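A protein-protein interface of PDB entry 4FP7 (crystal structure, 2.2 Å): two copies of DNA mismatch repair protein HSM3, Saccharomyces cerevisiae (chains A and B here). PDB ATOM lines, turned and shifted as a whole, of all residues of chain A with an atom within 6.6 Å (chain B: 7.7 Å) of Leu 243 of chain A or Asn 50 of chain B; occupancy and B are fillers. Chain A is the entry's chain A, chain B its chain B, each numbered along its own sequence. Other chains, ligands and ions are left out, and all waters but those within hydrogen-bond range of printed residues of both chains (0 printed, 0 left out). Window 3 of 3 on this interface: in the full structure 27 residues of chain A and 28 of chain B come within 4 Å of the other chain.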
ATOM      1  N   THR A 201     -26.344  11.005 -28.563  1.00  0.00           N
ATOM      2  CA  THR A 201     -26.487  11.965 -27.488  1.00  0.00           C
ATOM      3  C   THR A 201     -25.297  12.916 -27.313  1.00  0.00           C
ATOM      4  O   THR A 201     -25.479  14.122 -27.185  1.00  0.00           O
ATOM      5  CB  THR A 201     -26.784  11.244 -26.163  1.00  0.00           C
ATOM      6  OG1 THR A 201     -27.933  10.396 -26.329  1.00  0.00           O
ATOM      7  CG2 THR A 201     -27.067  12.244 -25.074  1.00  0.00           C
ATOM      8  N   VAL A 205     -25.464  16.978 -28.463  1.00  0.00           N
ATOM      9  CA  VAL A 205     -25.399  18.108 -27.550  1.00  0.00           C
ATOM     10  C   VAL A 205     -24.334  19.105 -28.020  1.00  0.00           C
ATOM     11  O   VAL A 205     -24.530  20.311 -27.953  1.00  0.00           O
ATOM     12  CB  VAL A 205     -25.102  17.647 -26.082  1.00  0.00           C
ATOM     13  CG1 VAL A 205     -24.794  18.834 -25.197  1.00  0.00           C
ATOM     14  CG2 VAL A 205     -26.284  16.873 -25.523  1.00  0.00           C
ATOM     15  N   SER A 238     -36.719  12.503 -31.327  1.00  0.00           N
ATOM     16  CA  SER A 238     -35.875  12.887 -30.196  1.00  0.00           C
ATOM     17  C   SER A 238     -36.475  12.466 -28.858  1.00  0.00           C
ATOM     18  O   SER A 238     -35.775  12.354 -27.858  1.00  0.00           O
ATOM     19  CB  SER A 238     -35.637  14.406 -30.207  1.00  0.00           C
ATOM     20  OG  SER A 238     -36.746  15.141 -29.682  1.00  0.00           O
ATOM     21  N   VAL A 239     -37.782  12.261 -28.832  1.00  0.00           N
ATOM     22  CA  VAL A 239     -38.442  11.901 -27.593  1.00  0.00           C
ATOM     23  C   VAL A 239     -37.940  10.554 -27.081  1.00  0.00           C
ATOM     24  O   VAL A 239     -37.929  10.307 -25.870  1.00  0.00           O
ATOM     25  CB  VAL A 239     -39.965  11.845 -27.757  1.00  0.00           C
ATOM     26  CG1 VAL A 239     -40.592  11.340 -26.490  1.00  0.00           C
ATOM     27  CG2 VAL A 239     -40.504  13.212 -28.106  1.00  0.00           C
ATOM     28  N   GLU A 240     -37.516   9.686 -27.994  1.00  0.00           N
ATOM     29  CA  GLU A 240     -36.969   8.377 -27.601  1.00  0.00           C
ATOM     30  C   GLU A 240     -35.865   8.477 -26.532  1.00  0.00           C
ATOM     31  O   GLU A 240     -35.742   7.596 -25.672  1.00  0.00           O
ATOM     32  CB  GLU A 240     -36.433   7.633 -28.824  1.00  0.00           C
ATOM     33  CG  GLU A 240     -37.517   7.166 -29.794  1.00  0.00           C
ATOM     34  CD  GLU A 240     -36.948   6.701 -31.134  1.00  0.00           C
ATOM     35  OE1 GLU A 240     -35.897   7.237 -31.558  1.00  0.00           O
ATOM     36  OE2 GLU A 240     -37.550   5.801 -31.761  1.00  0.00           O
ATOM     37  N   ASP A 241     -35.066   9.541 -26.587  1.00  0.00           N
ATOM     38  CA  ASP A 241     -34.035   9.786 -25.575  1.00  0.00           C
ATOM     39  C   ASP A 241     -34.299  11.124 -24.893  1.00  0.00           C
ATOM     40  O   ASP A 241     -33.733  12.142 -25.287  1.00  0.00           O
ATOM     41  CB  ASP A 241     -32.645   9.817 -26.221  1.00  0.00           C
ATOM     42  CG  ASP A 241     -31.525   9.942 -25.195  1.00  0.00           C
ATOM     43  OD1 ASP A 241     -31.835  10.192 -24.009  1.00  0.00           O
ATOM     44  OD2 ASP A 241     -30.337   9.788 -25.564  1.00  0.00           O
ATOM     45  N   ILE A 242     -35.145  11.128 -23.866  1.00  0.00           N
ATOM     46  CA  ILE A 242     -35.706  12.384 -23.363  1.00  0.00           C
ATOM     47  C   ILE A 242     -34.629  13.475 -23.189  1.00  0.00           C
ATOM     48  O   ILE A 242     -34.920  14.663 -23.271  1.00  0.00           O
ATOM     49  CB  ILE A 242     -36.508  12.174 -22.062  1.00  0.00           C
ATOM     50  CG1 ILE A 242     -37.483  13.343 -21.836  1.00  0.00           C
ATOM     51  CG2 ILE A 242     -35.564  11.982 -20.882  1.00  0.00           C
ATOM     52  CD1 ILE A 242     -38.515  13.536 -22.971  1.00  0.00           C
ATOM     53  N   LEU A 243     -33.385  13.056 -22.985  1.00  0.00           N
ATOM     54  CA  LEU A 243     -32.257  13.972 -22.849  1.00  0.00           C
ATOM     55  C   LEU A 243     -32.044  14.809 -24.137  1.00  0.00           C
ATOM     56  O   LEU A 243     -31.894  16.027 -24.087  1.00  0.00           O
ATOM     57  CB  LEU A 243     -31.021  13.133 -22.483  1.00  0.00           C
ATOM     58  CG  LEU A 243     -29.589  13.665 -22.524  1.00  0.00           C
ATOM     59  CD1 LEU A 243     -29.450  14.839 -21.626  1.00  0.00           C
ATOM     60  CD2 LEU A 243     -28.632  12.567 -22.094  1.00  0.00           C
ATOM     61  N   VAL A 244     -32.046  14.144 -25.284  1.00  0.00           N
ATOM     62  CA  VAL A 244     -31.971  14.818 -26.573  1.00  0.00           C
ATOM     63  C   VAL A 244     -33.168  15.774 -26.783  1.00  0.00           C
ATOM     64  O   VAL A 244     -32.997  16.932 -27.188  1.00  0.00           O
ATOM     65  CB  VAL A 244     -31.893  13.776 -27.717  1.00  0.00           C
ATOM     66  CG1 VAL A 244     -32.048  14.435 -29.064  1.00  0.00           C
ATOM     67  CG2 VAL A 244     -30.568  13.044 -27.649  1.00  0.00           C
ATOM     68  N   PHE A 245     -34.371  15.296 -26.477  1.00  0.00           N
ATOM     69  CA  PHE A 245     -35.568  16.114 -26.602  1.00  0.00           C
ATOM     70  C   PHE A 245     -35.419  17.402 -25.789  1.00  0.00           C
ATOM     71  O   PHE A 245     -35.676  18.491 -26.288  1.00  0.00           O
ATOM     72  CB  PHE A 245     -36.818  15.327 -26.180  1.00  0.00           C
ATOM     73  CG  PHE A 245     -38.069  16.160 -26.126  1.00  0.00           C
ATOM     74  CD1 PHE A 245     -38.731  16.501 -27.284  1.00  0.00           C
ATOM     75  CD2 PHE A 245     -38.568  16.618 -24.906  1.00  0.00           C
ATOM     76  CE1 PHE A 245     -39.857  17.277 -27.241  1.00  0.00           C
ATOM     77  CE2 PHE A 245     -39.702  17.385 -24.866  1.00  0.00           C
ATOM     78  CZ  PHE A 245     -40.353  17.713 -26.040  1.00  0.00           C
ATOM     79  N   ILE A 246     -34.971  17.269 -24.549  1.00  0.00           N
ATOM     80  CA  ILE A 246     -34.794  18.407 -23.670  1.00  0.00           C
ATOM     81  C   ILE A 246     -33.788  19.424 -24.250  1.00  0.00           C
ATOM     82  O   ILE A 246     -34.033  20.636 -24.215  1.00  0.00           O
ATOM     83  CB  ILE A 246     -34.365  17.923 -22.264  1.00  0.00           C
ATOM     84  CG1 ILE A 246     -35.570  17.285 -21.567  1.00  0.00           C
ATOM     85  CG2 ILE A 246     -33.839  19.088 -21.431  1.00  0.00           C
ATOM     86  CD1 ILE A 246     -35.234  16.436 -20.369  1.00  0.00           C
ATOM     87  N   GLU A 247     -32.678  18.934 -24.793  1.00  0.00           N
ATOM     88  CA  GLU A 247     -31.713  19.805 -25.472  1.00  0.00           C
ATOM     89  C   GLU A 247     -32.409  20.578 -26.578  1.00  0.00           C
ATOM     90  O   GLU A 247     -32.199  21.771 -26.754  1.00  0.00           O
ATOM     91  CB  GLU A 247     -30.569  18.976 -26.079  1.00  0.00           C
ATOM     92  CG  GLU A 247     -29.531  18.584 -25.065  1.00  0.00           C
ATOM     93  CD  GLU A 247     -28.533  19.698 -24.746  1.00  0.00           C
ATOM     94  OE1 GLU A 247     -28.080  20.414 -25.679  1.00  0.00           O
ATOM     95  OE2 GLU A 247     -28.197  19.842 -23.551  1.00  0.00           O
ATOM     96  N   LEU A 248     -33.277  19.877 -27.295  1.00  0.00           N
ATOM     97  CA  LEU A 248     -33.952  20.459 -28.425  1.00  0.00           C
ATOM     98  C   LEU A 248     -34.946  21.524 -27.957  1.00  0.00           C
ATOM     99  O   LEU A 248     -35.040  22.576 -28.573  1.00  0.00           O
ATOM    100  CB  LEU A 248     -34.624  19.355 -29.243  1.00  0.00           C
ATOM    101  CG  LEU A 248     -34.558  19.329 -30.777  1.00  0.00           C
ATOM    102  CD1 LEU A 248     -33.330  20.015 -31.414  1.00  0.00           C
ATOM    103  CD2 LEU A 248     -34.630  17.857 -31.207  1.00  0.00           C
ATOM    104  N   LEU B  43     -19.199   5.830 -17.892  1.00  0.00           N
ATOM    105  CA  LEU B  43     -20.396   5.891 -17.064  1.00  0.00           C
ATOM    106  C   LEU B  43     -20.484   7.234 -16.338  1.00  0.00           C
ATOM    107  O   LEU B  43     -21.568   7.806 -16.195  1.00  0.00           O
ATOM    108  CB  LEU B  43     -20.390   4.757 -16.037  1.00  0.00           C
ATOM    109  CG  LEU B  43     -21.663   4.619 -15.195  1.00  0.00           C
ATOM    110  CD1 LEU B  43     -22.891   4.364 -16.070  1.00  0.00           C
ATOM    111  CD2 LEU B  43     -21.510   3.510 -14.154  1.00  0.00           C
ATOM    112  N   LEU B  44     -19.334   7.726 -15.882  1.00  0.00           N
ATOM    113  CA  LEU B  44     -19.274   8.970 -15.125  1.00  0.00           C
ATOM    114  C   LEU B  44     -19.641  10.165 -16.000  1.00  0.00           C
ATOM    115  O   LEU B  44     -20.304  11.096 -15.542  1.00  0.00           O
ATOM    116  CB  LEU B  44     -17.884   9.159 -14.499  1.00  0.00           C
ATOM    117  CG  LEU B  44     -17.579   8.274 -13.284  1.00  0.00           C
ATOM    118  CD1 LEU B  44     -16.146   8.478 -12.795  1.00  0.00           C
ATOM    119  CD2 LEU B  44     -18.553   8.544 -12.168  1.00  0.00           C
ATOM    120  N   ARG B  45     -19.221  10.133 -17.261  1.00  0.00           N
ATOM    121  CA  ARG B  45     -19.602  11.171 -18.210  1.00  0.00           C
ATOM    122  C   ARG B  45     -21.093  11.063 -18.520  1.00  0.00           C
ATOM    123  O   ARG B  45     -21.790  12.073 -18.636  1.00  0.00           O
ATOM    124  CB  ARG B  45     -18.777  11.058 -19.493  1.00  0.00           C
ATOM    125  CG  ARG B  45     -17.296  11.335 -19.297  1.00  0.00           C
ATOM    126  CD  ARG B  45     -17.049  12.813 -19.047  1.00  0.00           C
ATOM    127  NE  ARG B  45     -16.705  13.527 -20.273  1.00  0.00           N
ATOM    128  CZ  ARG B  45     -16.756  14.850 -20.416  1.00  0.00           C
ATOM    129  NH1 ARG B  45     -17.155  15.624 -19.410  1.00  0.00           N
ATOM    130  NH2 ARG B  45     -16.415  15.400 -21.578  1.00  0.00           N
ATOM    131  N   LYS B  46     -21.583   9.832 -18.638  1.00  0.00           N
ATOM    132  CA  LYS B  46     -22.990   9.606 -18.932  1.00  0.00           C
ATOM    133  C   LYS B  46     -23.849  10.159 -17.786  1.00  0.00           C
ATOM    134  O   LYS B  46     -24.804  10.907 -18.012  1.00  0.00           O
ATOM    135  CB  LYS B  46     -23.257   8.110 -19.165  1.00  0.00           C
ATOM    136  CG  LYS B  46     -24.336   7.813 -20.214  1.00  0.00           C
ATOM    137  N   CYS B  47     -23.494   9.804 -16.557  1.00  0.00           N
ATOM    138  CA  CYS B  47     -24.193  10.323 -15.385  1.00  0.00           C
ATOM    139  C   CYS B  47     -24.233  11.853 -15.375  1.00  0.00           C
ATOM    140  O   CYS B  47     -25.280  12.449 -15.127  1.00  0.00           O
ATOM    141  CB  CYS B  47     -23.536   9.816 -14.099  1.00  0.00           C
ATOM    142  SG  CYS B  47     -23.863   8.076 -13.757  1.00  0.00           S
ATOM    143  N   SER B  48     -23.096  12.482 -15.643  1.00  0.00           N
ATOM    144  CA  SER B  48     -23.007  13.940 -15.591  1.00  0.00           C
ATOM    145  C   SER B  48     -23.914  14.600 -16.629  1.00  0.00           C
ATOM    146  O   SER B  48     -24.654  15.539 -16.305  1.00  0.00           O
ATOM    147  CB  SER B  48     -21.558  14.401 -15.770  1.00  0.00           C
ATOM    148  OG  SER B  48     -20.763  13.977 -14.673  1.00  0.00           O
ATOM    149  N   LEU B  49     -23.860  14.103 -17.864  1.00  0.00           N
ATOM    150  CA  LEU B  49     -24.696  14.637 -18.936  1.00  0.00           C
ATOM    151  C   LEU B  49     -26.169  14.463 -18.585  1.00  0.00           C
ATOM    152  O   LEU B  49     -26.952  15.418 -18.658  1.00  0.00           O
ATOM    153  CB  LEU B  49     -24.388  13.950 -20.271  1.00  0.00           C
ATOM    154  CG  LEU B  49     -25.066  14.578 -21.495  1.00  0.00           C
ATOM    155  CD1 LEU B  49     -24.787  16.080 -21.575  1.00  0.00           C
ATOM    156  CD2 LEU B  49     -24.613  13.889 -22.772  1.00  0.00           C
ATOM    157  N   ASN B  50     -26.533  13.247 -18.177  1.00  0.00           N
ATOM    158  CA  ASN B  50     -27.910  12.942 -17.804  1.00  0.00           C
ATOM    159  C   ASN B  50     -28.406  13.766 -16.617  1.00  0.00           C
ATOM    160  O   ASN B  50     -29.612  13.904 -16.420  1.00  0.00           O
ATOM    161  CB  ASN B  50     -28.073  11.449 -17.511  1.00  0.00           C
ATOM    162  CG  ASN B  50     -28.142  10.611 -18.777  1.00  0.00           C
ATOM    163  OD1 ASN B  50     -27.121  10.160 -19.293  1.00  0.00           O
ATOM    164  ND2 ASN B  50     -29.351  10.399 -19.283  1.00  0.00           N
ATOM    165  N   LEU B  51     -27.482  14.314 -15.832  1.00  0.00           N
ATOM    166  CA  LEU B  51     -27.856  15.174 -14.709  1.00  0.00           C
ATOM    167  C   LEU B  51     -27.915  16.657 -15.096  1.00  0.00           C
ATOM    168  O   LEU B  51     -28.785  17.373 -14.600  1.00  0.00           O
ATOM    169  CB  LEU B  51     -26.908  14.974 -13.513  1.00  0.00           C
ATOM    170  CG  LEU B  51     -26.950  13.622 -12.788  1.00  0.00           C
ATOM    171  CD1 LEU B  51     -25.865  13.575 -11.734  1.00  0.00           C
ATOM    172  CD2 LEU B  51     -28.313  13.322 -12.165  1.00  0.00           C
ATOM    173  N   VAL B  52     -27.002  17.127 -15.956  1.00  0.00           N
ATOM    174  CA  VAL B  52     -27.024  18.541 -16.376  1.00  0.00           C
ATOM    175  C   VAL B  52     -28.274  18.845 -17.194  1.00  0.00           C
ATOM    176  O   VAL B  52     -28.915  19.886 -17.011  1.00  0.00           O
ATOM    177  CB  VAL B  52     -25.786  19.009 -17.223  1.00  0.00           C
ATOM    178  CG1 VAL B  52     -24.577  19.330 -16.337  1.00  0.00           C
ATOM    179  CG2 VAL B  52     -25.436  18.004 -18.323  1.00  0.00           C
ATOM    180  N   THR B  53     -28.627  17.936 -18.094  1.00  0.00           N
ATOM    181  CA  THR B  53     -29.735  18.201 -18.991  1.00  0.00           C
ATOM    182  C   THR B  53     -31.066  18.039 -18.242  1.00  0.00           C
ATOM    183  O   THR B  53     -31.928  18.924 -18.291  1.00  0.00           O
ATOM    184  CB  THR B  53     -29.689  17.309 -20.245  1.00  0.00           C
ATOM    185  OG1 THR B  53     -28.369  17.338 -20.830  1.00  0.00           O
ATOM    186  CG2 THR B  53     -30.728  17.796 -21.268  1.00  0.00           C
ATOM    187  N   VAL B  54     -31.233  16.931 -17.527  1.00  0.00           N
ATOM    188  CA  VAL B  54     -32.457  16.756 -16.759  1.00  0.00           C
ATOM    189  C   VAL B  54     -32.348  17.558 -15.460  1.00  0.00           C
ATOM    190  O   VAL B  54     -32.536  17.025 -14.364  1.00  0.00           O
ATOM    191  CB  VAL B  54     -32.772  15.268 -16.468  1.00  0.00           C
ATOM    192  CG1 VAL B  54     -34.167  15.128 -15.867  1.00  0.00           C
ATOM    193  CG2 VAL B  54     -32.679  14.434 -17.744  1.00  0.00           C
ATOM    194  N   LYS B  93     -23.146  17.972  -9.837  1.00  0.00           N
ATOM    195  CA  LYS B  93     -24.440  18.068 -10.513  1.00  0.00           C
ATOM    196  C   LYS B  93     -25.536  17.424  -9.677  1.00  0.00           C
ATOM    197  O   LYS B  93     -26.715  17.700  -9.876  1.00  0.00           O
ATOM    198  CB  LYS B  93     -24.403  17.437 -11.915  1.00  0.00           C
ATOM    199  CG  LYS B  93     -23.363  18.029 -12.863  1.00  0.00           C
ATOM    200  CD  LYS B  93     -23.355  19.556 -12.826  1.00  0.00           C
ATOM    201  CE  LYS B  93     -22.075  20.121 -13.434  1.00  0.00           C
ATOM    202  NZ  LYS B  93     -21.993  21.608 -13.306  1.00  0.00           N
ATOM    203  N   MET B  97     -29.590  18.947  -6.496  1.00  0.00           N
ATOM    204  CA  MET B  97     -30.910  18.420  -6.822  1.00  0.00           C
ATOM    205  C   MET B  97     -31.461  17.532  -5.714  1.00  0.00           C
ATOM    206  O   MET B  97     -32.670  17.329  -5.606  1.00  0.00           O
ATOM    207  CB  MET B  97     -30.865  17.660  -8.150  1.00  0.00           C
ATOM    208  CG  MET B  97     -30.455  16.193  -8.047  1.00  0.00           C
ATOM    209  SD  MET B  97     -30.528  15.367  -9.652  1.00  0.00           S
ATOM    210  CE  MET B  97     -29.518  16.465 -10.672  1.00  0.00           C
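The side-chain hydroxyl (OG1) of Thr 201 of chain A is in hydrogen-bond range of the side-chain carboxylate (OD2) of Asp 241 of chain A (2.6 Å). The side-chain carboxylate of Asp 241 of chain A lies close to the backbone NH of Leu 243 of chain A (3.4 Å). The side-chain amide oxygen of Asn 50 of chain B lies close to the backbone carbonyl oxygen of Lys 46 of chain B (2.8 Å). The backbone carbonyl oxygen (O) of Leu 49 of chain B is in hydrogen-bond range of the side-chain hydroxyl (OG1) of Thr 53 of chain B, at 3.2 Å.
CD2 of Leu 49 of chain B touches CG2 of Thr 201 of chain A, 3.7 Å away. Leu 49 of chain B touches Leu 243 of chain A. Leu 243 of chain A touches Asn 50 of chain B. Thr 53 of chain B touches Leu 243 of chain A (OG1 to CD1, 2.8 Å). Ile 246 of chain A touches Thr 53 of chain B. OE2 of Glu 247 of chain A touches OG1 of Thr 53 of chain B, at 3.7 Å.
No position is printed for both chains.
Of the printed residues of chain B, Leu 243 of chain A touches Leu 49 (3.9 Å), Asn 50 (3.6 Å) and Thr 53 (2.8 Å). Ser 48 of chain B touches none of the printed residues of chain A. Printed residues of chain A within 4 Å of Leu 49 of chain B: Thr 201 and Leu 243. Printed residues of chain A within 4 Å of Thr 53 of chain B: Leu 243 (2.8 Å), Ile 246 (3.4 Å) and Glu 247 (3.7 Å). The nearest residue of chain B that does not touch Leu 243 of chain A is Val 54 of chain B (4.9 Å).
Hydrophobic or aromatic side chains of chain B that line the printed part of chain A: Leu 49. Of the 13 printed residues of chain A, 4 touch a printed residue of chain B. Hydrophobic or aromatic side chains of chain A within 4 Å of the printed part of chain B: Leu 243 and Ile 246. Among the printed residues, 6 pairs touch across the chains.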
